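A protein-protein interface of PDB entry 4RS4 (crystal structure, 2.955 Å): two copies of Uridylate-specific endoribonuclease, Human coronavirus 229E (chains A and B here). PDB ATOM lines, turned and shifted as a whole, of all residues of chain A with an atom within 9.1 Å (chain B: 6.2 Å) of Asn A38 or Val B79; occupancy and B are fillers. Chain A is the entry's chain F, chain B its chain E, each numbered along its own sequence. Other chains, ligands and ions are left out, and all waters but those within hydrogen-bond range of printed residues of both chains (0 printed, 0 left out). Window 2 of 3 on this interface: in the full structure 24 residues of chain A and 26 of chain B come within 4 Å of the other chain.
Printed residues of chain B within 4 Å of Asp A36: Lys B74 (3.4 Å). Val B78 touches none of the printed residues of chain A. Val B79 touches just one residue of chain A: Asn A38. Of the printed residues of chain A, Leu B95 touches Thr A39 (2.9 Å). No residue of chain A comes within 4 Å of Cys B113.
The backbone NH (N) of Val B79 sits at hydrogen-bond distance from the backbone carbonyl oxygen (O) of Cys B113, at 2.9 Å. The side-chain hydroxyl (OG1) of Thr B96 lies within hydrogen-bond range of the backbone carbonyl oxygen (O) of Phe B98 (2.6 Å).
Of the 8 printed residues of chain A, 3 touch a printed residue of chain B. Of the 16 printed residues of chain B, 5 touch a printed residue of chain A. Hydrophobic or aromatic side chains of chain B that line the printed part of chain A: Val B79. Among the printed residues, Asp or Glu carboxylates within 4 Å of a Lys or Arg side-chain nitrogen of the other chain: Asp A36 with Lys B74 (3.4 Å).
Val B79 touches Asn A38. CG2 of Thr A39 touches O of Leu B95, 2.9 Å away. Thr B96 touches Thr A39 (CA to CG2, 3.8 Å). CA of Thr A39 touches OG of Ser B97, 3.9 Å away.
The side-chain amino group (NZ) of Lys B74 is in salt-bridge range of the side-chain carboxylate (OD2) of Asp A36 (3.4 Å). The side-chain hydroxyl of Ser B97 sits at hydrogen-bond distance from the backbone carbonyl oxygen of Asn A38 (2.7 Å).
No position is printed for both chains.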
ATOM      1  N   VAL A  34     -13.084  -4.798  -2.242  1.00  0.00           N
ATOM      2  CA  VAL A  34     -14.065  -4.443  -1.215  1.00  0.00           C
ATOM      3  C   VAL A  34     -13.431  -3.484  -0.218  1.00  0.00           C
ATOM      4  O   VAL A  34     -12.272  -3.651   0.165  1.00  0.00           O
ATOM      5  CB  VAL A  34     -14.608  -5.669  -0.445  1.00  0.00           C
ATOM      6  CG1 VAL A  34     -15.318  -6.625  -1.395  1.00  0.00           C
ATOM      7  CG2 VAL A  34     -13.486  -6.374   0.300  1.00  0.00           C
ATOM      8  N   ARG A  35     -14.190  -2.485   0.214  1.00  0.00           N
ATOM      9  CA  ARG A  35     -13.660  -1.527   1.168  1.00  0.00           C
ATOM     10  C   ARG A  35     -13.949  -1.969   2.602  1.00  0.00           C
ATOM     11  O   ARG A  35     -15.101  -1.993   3.037  1.00  0.00           O
ATOM     12  CB  ARG A  35     -14.231  -0.129   0.912  1.00  0.00           C
ATOM     13  CG  ARG A  35     -13.941   0.854   2.026  1.00  0.00           C
ATOM     14  CD  ARG A  35     -14.368   2.267   1.675  1.00  0.00           C
ATOM     15  NE  ARG A  35     -14.088   3.181   2.781  1.00  0.00           N
ATOM     16  CZ  ARG A  35     -14.992   3.960   3.368  1.00  0.00           C
ATOM     17  NH1 ARG A  35     -16.251   3.960   2.951  1.00  0.00           N
ATOM     18  NH2 ARG A  35     -14.632   4.749   4.370  1.00  0.00           N
ATOM     19  N   ASP A  36     -12.889  -2.332   3.322  1.00  0.00           N
ATOM     20  CA  ASP A  36     -12.980  -2.635   4.743  1.00  0.00           C
ATOM     21  C   ASP A  36     -12.201  -1.591   5.538  1.00  0.00           C
ATOM     22  O   ASP A  36     -10.967  -1.563   5.502  1.00  0.00           O
ATOM     23  CB  ASP A  36     -12.441  -4.036   5.039  1.00  0.00           C
ATOM     24  CG  ASP A  36     -12.370  -4.332   6.529  1.00  0.00           C
ATOM     25  OD1 ASP A  36     -13.267  -3.869   7.273  1.00  0.00           O
ATOM     26  OD2 ASP A  36     -11.416  -5.023   6.952  1.00  0.00           O
ATOM     27  N   GLY A  37     -12.925  -0.745   6.266  1.00  0.00           N
ATOM     28  CA  GLY A  37     -12.310   0.344   7.002  1.00  0.00           C
ATOM     29  C   GLY A  37     -11.766   1.447   6.113  1.00  0.00           C
ATOM     30  O   GLY A  37     -12.488   1.996   5.279  1.00  0.00           O
ATOM     31  N   ASN A  38     -10.496   1.788   6.310  1.00  0.00           N
ATOM     32  CA  ASN A  38      -9.855   2.851   5.539  1.00  0.00           C
ATOM     33  C   ASN A  38      -9.067   2.361   4.329  1.00  0.00           C
ATOM     34  O   ASN A  38      -8.417   3.153   3.648  1.00  0.00           O
ATOM     35  CB  ASN A  38      -8.934   3.685   6.429  1.00  0.00           C
ATOM     36  CG  ASN A  38      -9.693   4.492   7.458  1.00  0.00           C
ATOM     37  OD1 ASN A  38      -9.582   4.244   8.657  1.00  0.00           O
ATOM     38  ND2 ASN A  38     -10.462   5.473   6.996  1.00  0.00           N
ATOM     39  N   THR A  39      -9.104   1.057   4.074  1.00  0.00           N
ATOM     40  CA  THR A  39      -8.354   0.491   2.959  1.00  0.00           C
ATOM     41  C   THR A  39      -9.227  -0.422   2.109  1.00  0.00           C
ATOM     42  O   THR A  39     -10.242  -0.945   2.576  1.00  0.00           O
ATOM     43  CB  THR A  39      -7.125  -0.302   3.450  1.00  0.00           C
ATOM     44  OG1 THR A  39      -7.513  -1.634   3.810  1.00  0.00           O
ATOM     45  CG2 THR A  39      -6.498   0.385   4.652  1.00  0.00           C
ATOM     46  N   ASP A  40      -8.831  -0.604   0.854  1.00  0.00           N
ATOM     47  CA  ASP A  40      -9.509  -1.550  -0.020  1.00  0.00           C
ATOM     48  C   ASP A  40      -8.739  -2.867  -0.067  1.00  0.00           C
ATOM     49  O   ASP A  40      -7.515  -2.877  -0.070  1.00  0.00           O
ATOM     50  CB  ASP A  40      -9.652  -0.985  -1.438  1.00  0.00           C
ATOM     51  CG  ASP A  40     -10.553   0.232  -1.499  1.00  0.00           C
ATOM     52  OD1 ASP A  40     -11.330   0.454  -0.548  1.00  0.00           O
ATOM     53  OD2 ASP A  40     -10.478   0.964  -2.506  1.00  0.00           O
ATOM     54  N   ASN A  41      -9.462  -3.974  -0.120  1.00  0.00           N
ATOM     55  CA  ASN A  41      -8.845  -5.284  -0.228  1.00  0.00           C
ATOM     56  C   ASN A  41      -9.098  -5.890  -1.594  1.00  0.00           C
ATOM     57  O   ASN A  41     -10.098  -5.590  -2.234  1.00  0.00           O
ATOM     58  CB  ASN A  41      -9.378  -6.211   0.857  1.00  0.00           C
ATOM     59  CG  ASN A  41      -8.534  -6.175   2.114  1.00  0.00           C
ATOM     60  OD1 ASN A  41      -7.304  -6.152   2.045  1.00  0.00           O
ATOM     61  ND2 ASN A  41      -9.187  -6.180   3.270  1.00  0.00           N
ATOM     62  N   LYS B  74      -3.881  -1.774  12.602  1.00  0.00           N
ATOM     63  CA  LYS B  74      -5.161  -1.709  11.911  1.00  0.00           C
ATOM     64  C   LYS B  74      -6.295  -1.657  12.929  1.00  0.00           C
ATOM     65  O   LYS B  74      -7.226  -0.862  12.791  1.00  0.00           O
ATOM     66  CB  LYS B  74      -5.352  -2.903  10.974  1.00  0.00           C
ATOM     67  CG  LYS B  74      -6.713  -2.919  10.285  1.00  0.00           C
ATOM     68  CD  LYS B  74      -7.068  -4.303   9.764  1.00  0.00           C
ATOM     69  CE  LYS B  74      -8.579  -4.485   9.669  1.00  0.00           C
ATOM     70  NZ  LYS B  74      -9.244  -3.372   8.928  1.00  0.00           N
ATOM     71  N   GLY B  77      -6.962   1.389  14.806  1.00  0.00           N
ATOM     72  CA  GLY B  77      -7.755   2.296  13.995  1.00  0.00           C
ATOM     73  C   GLY B  77      -6.980   3.341  13.213  1.00  0.00           C
ATOM     74  O   GLY B  77      -7.534   4.382  12.854  1.00  0.00           O
ATOM     75  N   VAL B  78      -5.707   3.070  12.936  1.00  0.00           N
ATOM     76  CA  VAL B  78      -4.874   4.034  12.224  1.00  0.00           C
ATOM     77  C   VAL B  78      -5.485   4.404  10.874  1.00  0.00           C
ATOM     78  O   VAL B  78      -5.690   3.542  10.022  1.00  0.00           O
ATOM     79  CB  VAL B  78      -3.467   3.459  11.971  1.00  0.00           C
ATOM     80  CG1 VAL B  78      -2.637   4.426  11.146  1.00  0.00           C
ATOM     81  CG2 VAL B  78      -2.779   3.123  13.288  1.00  0.00           C
ATOM     82  N   VAL B  79      -5.766   5.693  10.686  1.00  0.00           N
ATOM     83  CA  VAL B  79      -6.155   6.231   9.381  1.00  0.00           C
ATOM     84  C   VAL B  79      -4.960   6.576   8.491  1.00  0.00           C
ATOM     85  O   VAL B  79      -4.959   6.283   7.295  1.00  0.00           O
ATOM     86  CB  VAL B  79      -7.013   7.504   9.519  1.00  0.00           C
ATOM     87  CG1 VAL B  79      -7.301   8.110   8.146  1.00  0.00           C
ATOM     88  CG2 VAL B  79      -8.301   7.203  10.252  1.00  0.00           C
ATOM     89  N   ALA B  80      -3.950   7.214   9.080  1.00  0.00           N
ATOM     90  CA  ALA B  80      -2.835   7.753   8.302  1.00  0.00           C
ATOM     91  C   ALA B  80      -1.472   7.532   8.951  1.00  0.00           C
ATOM     92  O   ALA B  80      -1.381   7.157  10.121  1.00  0.00           O
ATOM     93  CB  ALA B  80      -3.054   9.230   8.024  1.00  0.00           C
ATOM     94  N   THR B  81      -0.418   7.763   8.169  1.00  0.00           N
ATOM     95  CA  THR B  81       0.958   7.607   8.633  1.00  0.00           C
ATOM     96  C   THR B  81       1.799   8.854   8.326  1.00  0.00           C
ATOM     97  O   THR B  81       1.622   9.496   7.285  1.00  0.00           O
ATOM     98  CB  THR B  81       1.619   6.346   8.032  1.00  0.00           C
ATOM     99  OG1 THR B  81       1.441   6.345   6.610  1.00  0.00           O
ATOM    100  CG2 THR B  81       0.987   5.089   8.613  1.00  0.00           C
ATOM    101  N   LEU B  95      -0.940   0.056   4.351  1.00  0.00           N
ATOM    102  CA  LEU B  95      -1.808  -0.232   5.485  1.00  0.00           C
ATOM    103  C   LEU B  95      -2.972   0.746   5.509  1.00  0.00           C
ATOM    104  O   LEU B  95      -4.014   0.480   6.111  1.00  0.00           O
ATOM    105  CB  LEU B  95      -1.020  -0.124   6.791  1.00  0.00           C
ATOM    106  CG  LEU B  95      -1.779  -0.395   8.089  1.00  0.00           C
ATOM    107  CD1 LEU B  95      -2.233  -1.843   8.146  1.00  0.00           C
ATOM    108  CD2 LEU B  95      -0.900  -0.060   9.278  1.00  0.00           C
ATOM    109  N   THR B  96      -2.777   1.877   4.838  1.00  0.00           N
ATOM    110  CA  THR B  96      -3.733   2.972   4.847  1.00  0.00           C
ATOM    111  C   THR B  96      -3.926   3.533   3.450  1.00  0.00           C
ATOM    112  O   THR B  96      -3.090   3.335   2.566  1.00  0.00           O
ATOM    113  CB  THR B  96      -3.220   4.131   5.707  1.00  0.00           C
ATOM    114  OG1 THR B  96      -2.064   4.710   5.084  1.00  0.00           O
ATOM    115  CG2 THR B  96      -2.854   3.649   7.101  1.00  0.00           C
ATOM    116  N   SER B  97      -5.030   4.243   3.259  1.00  0.00           N
ATOM    117  CA  SER B  97      -5.250   4.978   2.024  1.00  0.00           C
ATOM    118  C   SER B  97      -4.649   6.378   2.138  1.00  0.00           C
ATOM    119  O   SER B  97      -4.552   7.105   1.140  1.00  0.00           O
ATOM    120  CB  SER B  97      -6.748   5.065   1.712  1.00  0.00           C
ATOM    121  OG  SER B  97      -7.263   3.804   1.325  1.00  0.00           O
ATOM    122  N   PHE B  98      -4.235   6.747   3.352  1.00  0.00           N
ATOM    123  CA  PHE B  98      -3.844   8.128   3.639  1.00  0.00           C
ATOM    124  C   PHE B  98      -2.455   8.262   4.247  1.00  0.00           C
ATOM    125  O   PHE B  98      -1.942   7.322   4.853  1.00  0.00           O
ATOM    126  CB  PHE B  98      -4.863   8.788   4.561  1.00  0.00           C
ATOM    127  CG  PHE B  98      -6.238   8.902   3.966  1.00  0.00           C
ATOM    128  CD1 PHE B  98      -6.484   9.778   2.905  1.00  0.00           C
ATOM    129  CD2 PHE B  98      -7.295   8.150   4.480  1.00  0.00           C
ATOM    130  CE1 PHE B  98      -7.764   9.896   2.359  1.00  0.00           C
ATOM    131  CE2 PHE B  98      -8.578   8.258   3.941  1.00  0.00           C
ATOM    132  CZ  PHE B  98      -8.811   9.135   2.880  1.00  0.00           C
ATOM    133  N   THR B  99      -1.862   9.443   4.073  1.00  0.00           N
ATOM    134  CA  THR B  99      -0.517   9.741   4.556  1.00  0.00           C
ATOM    135  C   THR B  99      -0.451  11.179   5.043  1.00  0.00           C
ATOM    136  O   THR B  99      -1.336  11.988   4.767  1.00  0.00           O
ATOM    137  CB  THR B  99       0.544   9.588   3.445  1.00  0.00           C
ATOM    138  OG1 THR B  99       0.183  10.398   2.318  1.00  0.00           O
ATOM    139  CG2 THR B  99       0.678   8.143   3.006  1.00  0.00           C
ATOM    140  N   PHE B 108      -3.033  14.035   3.624  1.00  0.00           N
ATOM    141  CA  PHE B 108      -4.336  14.415   4.158  1.00  0.00           C
ATOM    142  C   PHE B 108      -4.193  15.527   5.203  1.00  0.00           C
ATOM    143  O   PHE B 108      -3.540  15.344   6.233  1.00  0.00           O
ATOM    144  CB  PHE B 108      -4.993  13.191   4.793  1.00  0.00           C
ATOM    145  CG  PHE B 108      -6.490  13.244   4.812  1.00  0.00           C
ATOM    146  CD1 PHE B 108      -7.173  14.162   4.034  1.00  0.00           C
ATOM    147  CD2 PHE B 108      -7.217  12.371   5.610  1.00  0.00           C
ATOM    148  CE1 PHE B 108      -8.555  14.209   4.049  1.00  0.00           C
ATOM    149  CE2 PHE B 108      -8.598  12.413   5.630  1.00  0.00           C
ATOM    150  CZ  PHE B 108      -9.268  13.334   4.848  1.00  0.00           C
ATOM    151  N   VAL B 112      -7.044  13.131  11.935  1.00  0.00           N
ATOM    152  CA  VAL B 112      -7.438  11.726  12.016  1.00  0.00           C
ATOM    153  C   VAL B 112      -6.428  10.976  12.871  1.00  0.00           C
ATOM    154  O   VAL B 112      -5.342  11.493  13.152  1.00  0.00           O
ATOM    155  CB  VAL B 112      -7.486  11.060  10.623  1.00  0.00           C
ATOM    156  CG1 VAL B 112      -8.499  11.754   9.729  1.00  0.00           C
ATOM    157  CG2 VAL B 112      -6.105  11.072   9.980  1.00  0.00           C
ATOM    158  N   CYS B 113      -6.770   9.752  13.264  1.00  0.00           N
ATOM    159  CA  CYS B 113      -5.867   8.951  14.081  1.00  0.00           C
ATOM    160  C   CYS B 113      -4.635   8.580  13.258  1.00  0.00           C
ATOM    161  O   CYS B 113      -4.742   7.955  12.203  1.00  0.00           O
ATOM    162  CB  CYS B 113      -6.580   7.694  14.581  1.00  0.00           C
ATOM    163  SG  CYS B 113      -5.503   6.512  15.428  1.00  0.00           S
ATOM    164  N   THR B 114      -3.463   8.958  13.756  1.00  0.00           N
ATOM    165  CA  THR B 114      -2.238   8.848  12.976  1.00  0.00           C
ATOM    166  C   THR B 114      -1.206   7.958  13.648  1.00  0.00           C
ATOM    167  O   THR B 114      -1.000   8.036  14.862  1.00  0.00           O
ATOM    168  CB  THR B 114      -1.606  10.232  12.743  1.00  0.00           C
ATOM    169  OG1 THR B 114      -2.534  11.077  12.046  1.00  0.00           O
ATOM    170  CG2 THR B 114      -0.306  10.109  11.938  1.00  0.00           C
ATOM    171  N   CYS B 115      -0.554   7.120  12.848  1.00  0.00           N
ATOM    172  CA  CYS B 115       0.514   6.274  13.349  1.00  0.00           C
ATOM    173  C   CYS B 115       1.842   7.004  13.195  1.00  0.00           C
ATOM    174  O   CYS B 115       2.075   7.665  12.182  1.00  0.00           O
ATOM    175  CB  CYS B 115       0.533   4.944  12.602  1.00  0.00           C
ATOM    176  SG  CYS B 115       1.678   3.732  13.289  1.00  0.00           S
